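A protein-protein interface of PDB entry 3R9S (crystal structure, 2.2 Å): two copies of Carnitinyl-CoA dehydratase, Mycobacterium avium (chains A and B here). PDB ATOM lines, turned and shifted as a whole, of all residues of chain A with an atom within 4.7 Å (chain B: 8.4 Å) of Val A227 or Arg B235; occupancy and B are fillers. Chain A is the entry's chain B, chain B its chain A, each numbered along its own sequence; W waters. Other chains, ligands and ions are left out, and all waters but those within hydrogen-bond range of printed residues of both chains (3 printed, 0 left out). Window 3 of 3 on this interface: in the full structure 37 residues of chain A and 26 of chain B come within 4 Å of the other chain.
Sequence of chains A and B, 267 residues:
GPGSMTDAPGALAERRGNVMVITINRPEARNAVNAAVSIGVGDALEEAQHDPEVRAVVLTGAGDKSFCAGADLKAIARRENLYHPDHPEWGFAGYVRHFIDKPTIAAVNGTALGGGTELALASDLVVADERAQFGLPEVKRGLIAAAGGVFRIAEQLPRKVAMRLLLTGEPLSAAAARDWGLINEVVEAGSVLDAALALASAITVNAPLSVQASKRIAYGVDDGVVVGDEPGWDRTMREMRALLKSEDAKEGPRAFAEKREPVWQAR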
ATOM      1  N   ILE A 217      13.485 -28.283 -12.801  1.00  0.00           N
ATOM      2  CA  ILE A 217      14.336 -27.137 -12.472  1.00  0.00           C
ATOM      3  C   ILE A 217      13.506 -25.859 -12.307  1.00  0.00           C
ATOM      4  O   ILE A 217      13.726 -25.095 -11.368  1.00  0.00           O
ATOM      5  CB  ILE A 217      15.430 -26.898 -13.498  1.00  0.00           C
ATOM      6  CG1 ILE A 217      16.385 -28.098 -13.547  1.00  0.00           C
ATOM      7  CG2 ILE A 217      16.206 -25.626 -13.151  1.00  0.00           C
ATOM      8  CD1 ILE A 217      17.164 -28.251 -14.858  1.00  0.00           C
ATOM      9  N   GLY A 220      12.042 -25.763  -8.915  1.00  0.00           N
ATOM     10  CA  GLY A 220      12.945 -26.051  -7.802  1.00  0.00           C
ATOM     11  C   GLY A 220      12.625 -27.381  -7.116  1.00  0.00           C
ATOM     12  O   GLY A 220      12.499 -27.447  -5.904  1.00  0.00           O
ATOM     13  N   VAL A 221      12.482 -28.439  -7.902  1.00  0.00           N
ATOM     14  CA  VAL A 221      12.100 -29.732  -7.377  1.00  0.00           C
ATOM     15  C   VAL A 221      13.320 -30.569  -6.962  1.00  0.00           C
ATOM     16  O   VAL A 221      14.240 -30.783  -7.746  1.00  0.00           O
ATOM     17  CB  VAL A 221      11.223 -30.494  -8.386  1.00  0.00           C
ATOM     18  CG1 VAL A 221      11.013 -31.936  -7.938  1.00  0.00           C
ATOM     19  CG2 VAL A 221       9.860 -29.791  -8.525  1.00  0.00           C
ATOM     20  N   ASP A 222      13.319 -30.982  -5.695  1.00  0.00           N
ATOM     21  CA  ASP A 222      14.247 -31.956  -5.153  1.00  0.00           C
ATOM     22  C   ASP A 222      13.416 -33.151  -4.685  1.00  0.00           C
ATOM     23  O   ASP A 222      12.497 -32.998  -3.881  1.00  0.00           O
ATOM     24  CB  ASP A 222      15.031 -31.371  -3.969  1.00  0.00           C
ATOM     25  CG  ASP A 222      15.888 -30.179  -4.363  1.00  0.00           C
ATOM     26  OD1 ASP A 222      16.493 -30.203  -5.463  1.00  0.00           O
ATOM     27  OD2 ASP A 222      15.959 -29.216  -3.567  1.00  0.00           O
ATOM     28  N   VAL A 225       9.627 -33.103  -4.630  1.00  0.00           N
ATOM     29  CA  VAL A 225       8.992 -32.048  -3.806  1.00  0.00           C
ATOM     30  C   VAL A 225       9.333 -30.647  -4.283  1.00  0.00           C
ATOM     31  O   VAL A 225      10.509 -30.308  -4.453  1.00  0.00           O
ATOM     32  CB  VAL A 225       9.405 -32.123  -2.328  1.00  0.00           C
ATOM     33  CG1 VAL A 225       8.671 -31.037  -1.540  1.00  0.00           C
ATOM     34  CG2 VAL A 225       9.123 -33.517  -1.753  1.00  0.00           C
ATOM     35  N   VAL A 226       8.301 -29.828  -4.473  1.00  0.00           N
ATOM     36  CA  VAL A 226       8.483 -28.409  -4.784  1.00  0.00           C
ATOM     37  C   VAL A 226       8.881 -27.700  -3.484  1.00  0.00           C
ATOM     38  O   VAL A 226       8.014 -27.293  -2.703  1.00  0.00           O
ATOM     39  CB  VAL A 226       7.201 -27.797  -5.385  1.00  0.00           C
ATOM     40  CG1 VAL A 226       7.407 -26.301  -5.730  1.00  0.00           C
ATOM     41  CG2 VAL A 226       6.745 -28.598  -6.618  1.00  0.00           C
ATOM     42  N   VAL A 227      10.187 -27.547  -3.252  1.00  0.00           N
ATOM     43  CA  VAL A 227      10.671 -27.170  -1.911  1.00  0.00           C
ATOM     44  C   VAL A 227      10.191 -25.788  -1.515  1.00  0.00           C
ATOM     45  O   VAL A 227       9.896 -25.564  -0.359  1.00  0.00           O
ATOM     46  CB  VAL A 227      12.231 -27.274  -1.732  1.00  0.00           C
ATOM     47  CG1 VAL A 227      12.727 -28.654  -2.114  1.00  0.00           C
ATOM     48  CG2 VAL A 227      12.964 -26.220  -2.525  1.00  0.00           C
ATOM     49  N   GLY A 228      10.096 -24.877  -2.478  1.00  0.00           N
ATOM     50  CA  GLY A 228       9.636 -23.510  -2.238  1.00  0.00           C
ATOM     51  C   GLY A 228       8.164 -23.350  -1.854  1.00  0.00           C
ATOM     52  O   GLY A 228       7.774 -22.281  -1.390  1.00  0.00           O
ATOM     53  N   ASP A 229       7.362 -24.398  -2.062  1.00  0.00           N
ATOM     54  CA  ASP A 229       5.953 -24.414  -1.678  1.00  0.00           C
ATOM     55  C   ASP A 229       5.746 -24.779  -0.204  1.00  0.00           C
ATOM     56  O   ASP A 229       4.713 -24.442   0.372  1.00  0.00           O
ATOM     57  CB  ASP A 229       5.157 -25.443  -2.498  1.00  0.00           C
ATOM     58  CG  ASP A 229       4.795 -24.966  -3.883  1.00  0.00           C
ATOM     59  OD1 ASP A 229       5.083 -23.807  -4.239  1.00  0.00           O
ATOM     60  OD2 ASP A 229       4.202 -25.787  -4.622  1.00  0.00           O
ATOM     61  N   GLU A 230       6.701 -25.486   0.391  1.00  0.00           N
ATOM     62  CA  GLU A 230       6.497 -26.033   1.744  1.00  0.00           C
ATOM     63  C   GLU A 230       6.159 -24.974   2.810  1.00  0.00           C
ATOM     64  O   GLU A 230       5.246 -25.188   3.600  1.00  0.00           O
ATOM     65  CB  GLU A 230       7.689 -26.901   2.183  1.00  0.00           C
ATOM     66  CG  GLU A 230       7.893 -28.139   1.290  1.00  0.00           C
ATOM     67  CD  GLU A 230       6.696 -29.095   1.314  1.00  0.00           C
ATOM     68  OE1 GLU A 230       5.874 -29.090   0.370  1.00  0.00           O
ATOM     69  OE2 GLU A 230       6.568 -29.855   2.299  1.00  0.00           O
ATOM     70  N   PRO A 231       6.874 -23.826   2.818  1.00  0.00           N
ATOM     71  CA  PRO A 231       6.469 -22.772   3.770  1.00  0.00           C
ATOM     72  C   PRO A 231       5.035 -22.258   3.528  1.00  0.00           C
ATOM     73  O   PRO A 231       4.339 -21.912   4.476  1.00  0.00           O
ATOM     74  CB  PRO A 231       7.507 -21.661   3.546  1.00  0.00           C
ATOM     75  CG  PRO A 231       8.698 -22.355   2.966  1.00  0.00           C
ATOM     76  CD  PRO A 231       8.122 -23.485   2.119  1.00  0.00           C
ATOM     77  N   ILE B 144      18.610 -28.986 -22.823  1.00  0.00           N
ATOM     78  CA  ILE B 144      17.867 -28.045 -22.010  1.00  0.00           C
ATOM     79  C   ILE B 144      18.551 -26.671 -21.998  1.00  0.00           C
ATOM     80  O   ILE B 144      19.698 -26.530 -22.431  1.00  0.00           O
ATOM     81  CB  ILE B 144      17.646 -28.551 -20.570  1.00  0.00           C
ATOM     82  CG1 ILE B 144      18.991 -28.808 -19.867  1.00  0.00           C
ATOM     83  CG2 ILE B 144      16.742 -29.825 -20.565  1.00  0.00           C
ATOM     84  CD1 ILE B 144      18.894 -28.945 -18.362  1.00  0.00           C
ATOM     85  N   ALA B 146      20.381 -24.825 -20.229  1.00  0.00           N
ATOM     86  CA  ALA B 146      21.299 -25.012 -19.130  1.00  0.00           C
ATOM     87  C   ALA B 146      22.086 -23.753 -18.764  1.00  0.00           C
ATOM     88  O   ALA B 146      22.747 -23.738 -17.747  1.00  0.00           O
ATOM     89  CB  ALA B 146      22.296 -26.143 -19.493  1.00  0.00           C
ATOM     90  N   VAL B 150      16.390 -22.269 -17.791  1.00  0.00           N
ATOM     91  CA  VAL B 150      15.403 -23.114 -17.115  1.00  0.00           C
ATOM     92  C   VAL B 150      14.897 -22.556 -15.805  1.00  0.00           C
ATOM     93  O   VAL B 150      13.770 -22.847 -15.448  1.00  0.00           O
ATOM     94  CB  VAL B 150      15.881 -24.587 -16.851  1.00  0.00           C
ATOM     95  CG1 VAL B 150      15.743 -25.418 -18.093  1.00  0.00           C
ATOM     96  CG2 VAL B 150      17.326 -24.641 -16.307  1.00  0.00           C
ATOM     97  N   PHE B 151      15.717 -21.804 -15.066  1.00  0.00           N
ATOM     98  CA  PHE B 151      15.235 -21.179 -13.819  1.00  0.00           C
ATOM     99  C   PHE B 151      15.050 -19.672 -13.919  1.00  0.00           C
ATOM    100  O   PHE B 151      14.379 -19.096 -13.064  1.00  0.00           O
ATOM    101  CB  PHE B 151      16.112 -21.541 -12.595  1.00  0.00           C
ATOM    102  CG  PHE B 151      17.549 -21.099 -12.697  1.00  0.00           C
ATOM    103  CD1 PHE B 151      18.525 -21.967 -13.171  1.00  0.00           C
ATOM    104  CD2 PHE B 151      17.930 -19.832 -12.296  1.00  0.00           C
ATOM    105  CE1 PHE B 151      19.852 -21.575 -13.243  1.00  0.00           C
ATOM    106  CE2 PHE B 151      19.255 -19.431 -12.385  1.00  0.00           C
ATOM    107  CZ  PHE B 151      20.216 -20.315 -12.854  1.00  0.00           C
ATOM    108  N   GLY B 228      20.688 -16.313  -4.645  1.00  0.00           N
ATOM    109  CA  GLY B 228      19.416 -16.932  -5.022  1.00  0.00           C
ATOM    110  C   GLY B 228      19.478 -17.808  -6.274  1.00  0.00           C
ATOM    111  O   GLY B 228      18.622 -18.647  -6.467  1.00  0.00           O
ATOM    112  N   ASP B 229      20.483 -17.602  -7.126  1.00  0.00           N
ATOM    113  CA  ASP B 229      20.670 -18.394  -8.352  1.00  0.00           C
ATOM    114  C   ASP B 229      21.338 -19.746  -8.104  1.00  0.00           C
ATOM    115  O   ASP B 229      21.263 -20.649  -8.936  1.00  0.00           O
ATOM    116  CB  ASP B 229      21.532 -17.630  -9.363  1.00  0.00           C
ATOM    117  CG  ASP B 229      20.781 -16.508 -10.088  1.00  0.00           C
ATOM    118  OD1 ASP B 229      19.540 -16.373  -9.966  1.00  0.00           O
ATOM    119  OD2 ASP B 229      21.467 -15.765 -10.824  1.00  0.00           O
ATOM    120  N   GLU B 230      22.005 -19.890  -6.969  1.00  0.00           N
ATOM    121  CA  GLU B 230      22.844 -21.058  -6.757  1.00  0.00           C
ATOM    122  C   GLU B 230      22.050 -22.362  -6.749  1.00  0.00           C
ATOM    123  O   GLU B 230      22.518 -23.356  -7.306  1.00  0.00           O
ATOM    124  CB  GLU B 230      23.699 -20.901  -5.492  1.00  0.00           C
ATOM    125  CG  GLU B 230      24.761 -19.806  -5.644  1.00  0.00           C
ATOM    126  CD  GLU B 230      25.780 -20.130  -6.744  1.00  0.00           C
ATOM    127  OE1 GLU B 230      25.759 -19.475  -7.823  1.00  0.00           O
ATOM    128  OE2 GLU B 230      26.577 -21.071  -6.542  1.00  0.00           O
ATOM    129  N   PRO B 231      20.859 -22.373  -6.129  1.00  0.00           N
ATOM    130  CA  PRO B 231      20.093 -23.620  -6.214  1.00  0.00           C
ATOM    131  C   PRO B 231      19.669 -23.983  -7.647  1.00  0.00           C
ATOM    132  O   PRO B 231      19.593 -25.173  -7.964  1.00  0.00           O
ATOM    133  CB  PRO B 231      18.871 -23.354  -5.310  1.00  0.00           C
ATOM    134  CG  PRO B 231      19.350 -22.322  -4.340  1.00  0.00           C
ATOM    135  CD  PRO B 231      20.258 -21.434  -5.162  1.00  0.00           C
ATOM    136  N   GLY B 232      19.439 -22.981  -8.500  1.00  0.00           N
ATOM    137  CA  GLY B 232      19.082 -23.224  -9.892  1.00  0.00           C
ATOM    138  C   GLY B 232      20.238 -23.805 -10.691  1.00  0.00           C
ATOM    139  O   GLY B 232      20.056 -24.736 -11.475  1.00  0.00           O
ATOM    140  N   TRP B 233      21.427 -23.241 -10.510  1.00  0.00           N
ATOM    141  CA  TRP B 233      22.633 -23.783 -11.122  1.00  0.00           C
ATOM    142  C   TRP B 233      22.909 -25.210 -10.645  1.00  0.00           C
ATOM    143  O   TRP B 233      23.181 -26.074 -11.452  1.00  0.00           O
ATOM    144  CB  TRP B 233      23.841 -22.918 -10.786  1.00  0.00           C
ATOM    145  CG  TRP B 233      23.829 -21.589 -11.446  1.00  0.00           C
ATOM    146  CD1 TRP B 233      23.884 -20.381 -10.834  1.00  0.00           C
ATOM    147  CD2 TRP B 233      23.762 -21.329 -12.845  1.00  0.00           C
ATOM    148  NE1 TRP B 233      23.876 -19.376 -11.761  1.00  0.00           N
ATOM    149  CE2 TRP B 233      23.798 -19.932 -13.009  1.00  0.00           C
ATOM    150  CE3 TRP B 233      23.680 -22.143 -13.988  1.00  0.00           C
ATOM    151  CZ2 TRP B 233      23.745 -19.327 -14.268  1.00  0.00           C
ATOM    152  CZ3 TRP B 233      23.647 -21.546 -15.232  1.00  0.00           C
ATOM    153  CH2 TRP B 233      23.666 -20.147 -15.362  1.00  0.00           C
ATOM    154  N   ASP B 234      22.825 -25.440  -9.338  1.00  0.00           N
ATOM    155  CA  ASP B 234      23.077 -26.761  -8.763  1.00  0.00           C
ATOM    156  C   ASP B 234      22.112 -27.808  -9.347  1.00  0.00           C
ATOM    157  O   ASP B 234      22.535 -28.889  -9.756  1.00  0.00           O
ATOM    158  CB  ASP B 234      22.979 -26.727  -7.223  1.00  0.00           C
ATOM    159  CG  ASP B 234      24.117 -25.927  -6.557  1.00  0.00           C
ATOM    160  OD1 ASP B 234      25.141 -25.614  -7.220  1.00  0.00           O
ATOM    161  OD2 ASP B 234      23.990 -25.625  -5.343  1.00  0.00           O
ATOM    162  N   ARG B 235      20.826 -27.474  -9.420  1.00  0.00           N
ATOM    163  CA  ARG B 235      19.838 -28.389  -9.999  1.00  0.00           C
ATOM    164  C   ARG B 235      20.034 -28.588 -11.488  1.00  0.00           C
ATOM    165  O   ARG B 235      19.753 -29.666 -11.999  1.00  0.00           O
ATOM    166  CB  ARG B 235      18.413 -27.897  -9.770  1.00  0.00           C
ATOM    167  CG  ARG B 235      17.965 -28.006  -8.362  1.00  0.00           C
ATOM    168  CD  ARG B 235      16.494 -27.773  -8.231  1.00  0.00           C
ATOM    169  NE  ARG B 235      16.130 -27.642  -6.830  1.00  0.00           N
ATOM    170  CZ  ARG B 235      15.974 -26.498  -6.176  1.00  0.00           C
ATOM    171  NH1 ARG B 235      16.107 -25.323  -6.777  1.00  0.00           N
ATOM    172  NH2 ARG B 235      15.640 -26.529  -4.901  1.00  0.00           N
ATOM    173  N   THR B 236      20.443 -27.532 -12.187  1.00  0.00           N
ATOM    174  CA  THR B 236      20.722 -27.617 -13.605  1.00  0.00           C
ATOM    175  C   THR B 236      21.873 -28.601 -13.854  1.00  0.00           C
ATOM    176  O   THR B 236      21.787 -29.426 -14.754  1.00  0.00           O
ATOM    177  CB  THR B 236      21.071 -26.232 -14.223  1.00  0.00           C
ATOM    178  OG1 THR B 236      19.953 -25.330 -14.103  1.00  0.00           O
ATOM    179  CG2 THR B 236      21.429 -26.379 -15.705  1.00  0.00           C
ATOM    180  N   MET B 237      22.926 -28.524 -13.033  1.00  0.00           N
ATOM    181  CA  MET B 237      24.085 -29.403 -13.169  1.00  0.00           C
ATOM    182  C   MET B 237      23.682 -30.850 -12.867  1.00  0.00           C
ATOM    183  O   MET B 237      23.996 -31.758 -13.636  1.00  0.00           O
ATOM    184  CB  MET B 237      25.244 -28.937 -12.258  1.00  0.00           C
ATOM    185  CG  MET B 237      25.898 -27.603 -12.747  1.00  0.00           C
ATOM    186  SD  MET B 237      27.413 -27.036 -11.888  1.00  0.00           S
ATOM    187  CE  MET B 237      26.704 -25.917 -10.660  1.00  0.00           C
ATOM    188  N   ARG B 238      22.953 -31.030 -11.769  1.00  0.00           N
ATOM    189  CA  ARG B 238      22.459 -32.337 -11.347  1.00  0.00           C
ATOM    190  C   ARG B 238      21.652 -33.025 -12.461  1.00  0.00           C
ATOM    191  O   ARG B 238      21.911 -34.181 -12.774  1.00  0.00           O
ATOM    192  CB  ARG B 238      21.614 -32.179 -10.080  1.00  0.00           C
ATOM    193  CG  ARG B 238      21.212 -33.469  -9.412  1.00  0.00           C
ATOM    194  CD  ARG B 238      20.271 -33.181  -8.254  1.00  0.00           C
ATOM    195  NE  ARG B 238      18.942 -32.773  -8.727  1.00  0.00           N
ATOM    196  CZ  ARG B 238      18.059 -32.054  -8.030  1.00  0.00           C
ATOM    197  NH1 ARG B 238      18.325 -31.629  -6.799  1.00  0.00           N
ATOM    198  NH2 ARG B 238      16.888 -31.757  -8.580  1.00  0.00           N
ATOM    199  N   GLU B 239      20.709 -32.301 -13.068  1.00  0.00           N
ATOM    200  CA  GLU B 239      19.865 -32.846 -14.145  1.00  0.00           C
ATOM    201  C   GLU B 239      20.661 -33.212 -15.405  1.00  0.00           C
ATOM    202  O   GLU B 239      20.455 -34.277 -15.991  1.00  0.00           O
ATOM    203  CB  GLU B 239      18.772 -31.843 -14.539  1.00  0.00           C
ATOM    204  CG  GLU B 239      17.761 -31.550 -13.439  1.00  0.00           C
ATOM    205  CD  GLU B 239      16.754 -32.658 -13.229  1.00  0.00           C
ATOM    206  OE1 GLU B 239      16.752 -33.638 -13.999  1.00  0.00           O
ATOM    207  OE2 GLU B 239      15.951 -32.550 -12.296  1.00  0.00           O
ATOM    208  N   MET B 240      21.542 -32.304 -15.814  1.00  0.00           N
ATOM    209  CA  MET B 240      22.385 -32.458 -17.009  1.00  0.00           C
ATOM    210  C   MET B 240      23.112 -33.804 -17.019  1.00  0.00           C
ATOM    211  O   MET B 240      23.218 -34.467 -18.046  1.00  0.00           O
ATOM    212  CB  MET B 240      23.422 -31.324 -17.049  1.00  0.00           C
ATOM    213  CG  MET B 240      23.514 -30.594 -18.360  1.00  0.00           C
ATOM    214  SD  MET B 240      23.831 -28.820 -18.128  1.00  0.00           S
ATOM    215  CE  MET B 240      25.133 -28.772 -16.907  1.00  0.00           C
ATOM    216  N   ARG B 241      23.628 -34.180 -15.861  1.00  0.00           N
ATOM    217  CA  ARG B 241      24.328 -35.444 -15.705  1.00  0.00           C
ATOM    218  C   ARG B 241      23.461 -36.670 -16.015  1.00  0.00           C
ATOM    219  O   ARG B 241      23.943 -37.601 -16.663  1.00  0.00           O
ATOM    220  CB  ARG B 241      24.952 -35.541 -14.302  1.00  0.00           C
ATOM    221  CG  ARG B 241      26.397 -34.967 -14.244  1.00  0.00           C
ATOM    222  CD  ARG B 241      26.699 -34.253 -12.925  1.00  0.00           C
ATOM    223  NE  ARG B 241      26.055 -34.921 -11.793  1.00  0.00           N
ATOM    224  CZ  ARG B 241      25.688 -34.320 -10.660  1.00  0.00           C
ATOM    225  NH1 ARG B 241      25.907 -33.014 -10.467  1.00  0.00           N
ATOM    226  NH2 ARG B 241      25.093 -35.037  -9.704  1.00  0.00           N
ATOM    227  N   ALA B 242      22.198 -36.680 -15.571  1.00  0.00           N
ATOM    228  CA  ALA B 242      21.297 -37.800 -15.905  1.00  0.00           C
ATOM    229  C   ALA B 242      20.914 -37.791 -17.383  1.00  0.00           C
ATOM    230  O   ALA B 242      20.835 -38.852 -18.007  1.00  0.00           O
ATOM    231  CB  ALA B 242      20.043 -37.788 -15.033  1.00  0.00           C
ATOM    232  N   LEU B 243      20.709 -36.599 -17.949  1.00  0.00           N
ATOM    233  CA  LEU B 243      20.330 -36.474 -19.364  1.00  0.00           C
ATOM    234  C   LEU B 243      21.410 -36.986 -20.314  1.00  0.00           C
ATOM    235  O   LEU B 243      21.096 -37.659 -21.304  1.00  0.00           O
ATOM    236  CB  LEU B 243      19.954 -35.028 -19.721  1.00  0.00           C
ATOM    237  CG  LEU B 243      18.649 -34.521 -19.083  1.00  0.00           C
ATOM    238  CD1 LEU B 243      18.583 -33.003 -19.144  1.00  0.00           C
ATOM    239  CD2 LEU B 243      17.397 -35.154 -19.722  1.00  0.00           C
HETATM  240  O   HOH W   1      15.697 -24.539  -9.471  1.00  0.00           O
HETATM  241  O   HOH W   2      15.696 -30.569 -10.412  1.00  0.00           O
HETATM  242  O   HOH W   3      14.634 -33.963  -8.587  1.00  0.00           O
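Of the 20 printed residues of chain B, 6 touch a printed residue of chain A. Printed residues of chain B that touch a printed residue of chain A: Ile B144, Val B150, Arg B235, Thr B236, Arg B238 and Glu B239. Of the 11 printed residues of chain A, 5 touch a printed residue of chain B. Hydrophobic or aromatic side chains of chain A that line the printed part of chain B: Ile A217 and Val A227. Among the printed residues, Asp or Glu carboxylates within 4 Å of a Lys or Arg side-chain nitrogen of the other chain: Asp A222 with Arg B235 (2.9 Å) and Asp A222 with Arg B238 (2.7 Å).
Among the printed residues, merely in contact across the chains: Ile A217 with Ile B144 (3.97 Å), Ile A217 with Val B150 (3.5 Å), Ile A217 with Thr B236 (3.8 Å), Ile A217 with Glu B239 (3.6 Å), Val A221 with Arg B235 (3.8 Å) and Val A227 with Arg B235 (3.6 Å).
The guanidinium group (NH2) of Arg B238 is in salt-bridge range of the side-chain carboxylate (OE2) of Glu B239, 3.9 Å away. The side-chain hydroxyl (OG1) of Thr B236 sits at hydrogen-bond distance from the backbone carbonyl oxygen (O) of Gly B232, 2.7 Å away.
Water W2 lies within hydrogen-bond range of the guanidinium group of Arg B238 (2.5 Å), the side-chain carboxylate of Glu B239 (2.7 Å) and the backbone carbonyl oxygen of Val A221 (3.0 Å). Water W1 lies within hydrogen-bond range of the backbone carbonyl oxygen (O) of Ile A217 (2.8 Å) and the guanidinium group (NH1) of Arg B235 (2.8 Å). Water W3 lies within hydrogen-bond range of the guanidinium group (NH2) of Arg B238 (3.2 Å) and the backbone carbonyl oxygen (O) of Val A221 (3.3 Å).
Of the printed residues of chain B, Asp A222 touches Arg B235 and Arg B238. Val A227 touches just one residue of chain B: Arg B235 (3.6 Å). No residue of chain B comes within 4 Å of Gly A228. Pro A231 touches none of the printed residues of chain B. Of the printed residues of chain A, Val B150 touches Ile A217 (3.5 Å). Gly B232 touches none of the printed residues of chain A. Of chain A, only Gly A220, Val A221, Asp A222 and Val A227 come within 4 Å of Arg B235. The nearest printed residue of chain A that does not touch Thr B236 is Asp A222 (8.2 Å).
Positions printed for both chains: 228, 229, 230 and 231. Of the 10 pairs that touch across the chains among the printed residues, none has its exchanged pair printed and touching as well.
The guanidinium group (NE) of Arg B235 lies within salt-bridge range of the side-chain carboxylate (OD1) of Asp A222 (2.9 Å). O of Val A221 is in hydrogen-bond range of NH2 of Arg B238, at 2.9 Å. NH2 of Arg B235 is in hydrogen-bond range of O of Gly A220, at 3.4 Å. The side-chain carboxylate of Asp A222 lies within salt-bridge range of the guanidinium group of Arg B238 (2.7 Å).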
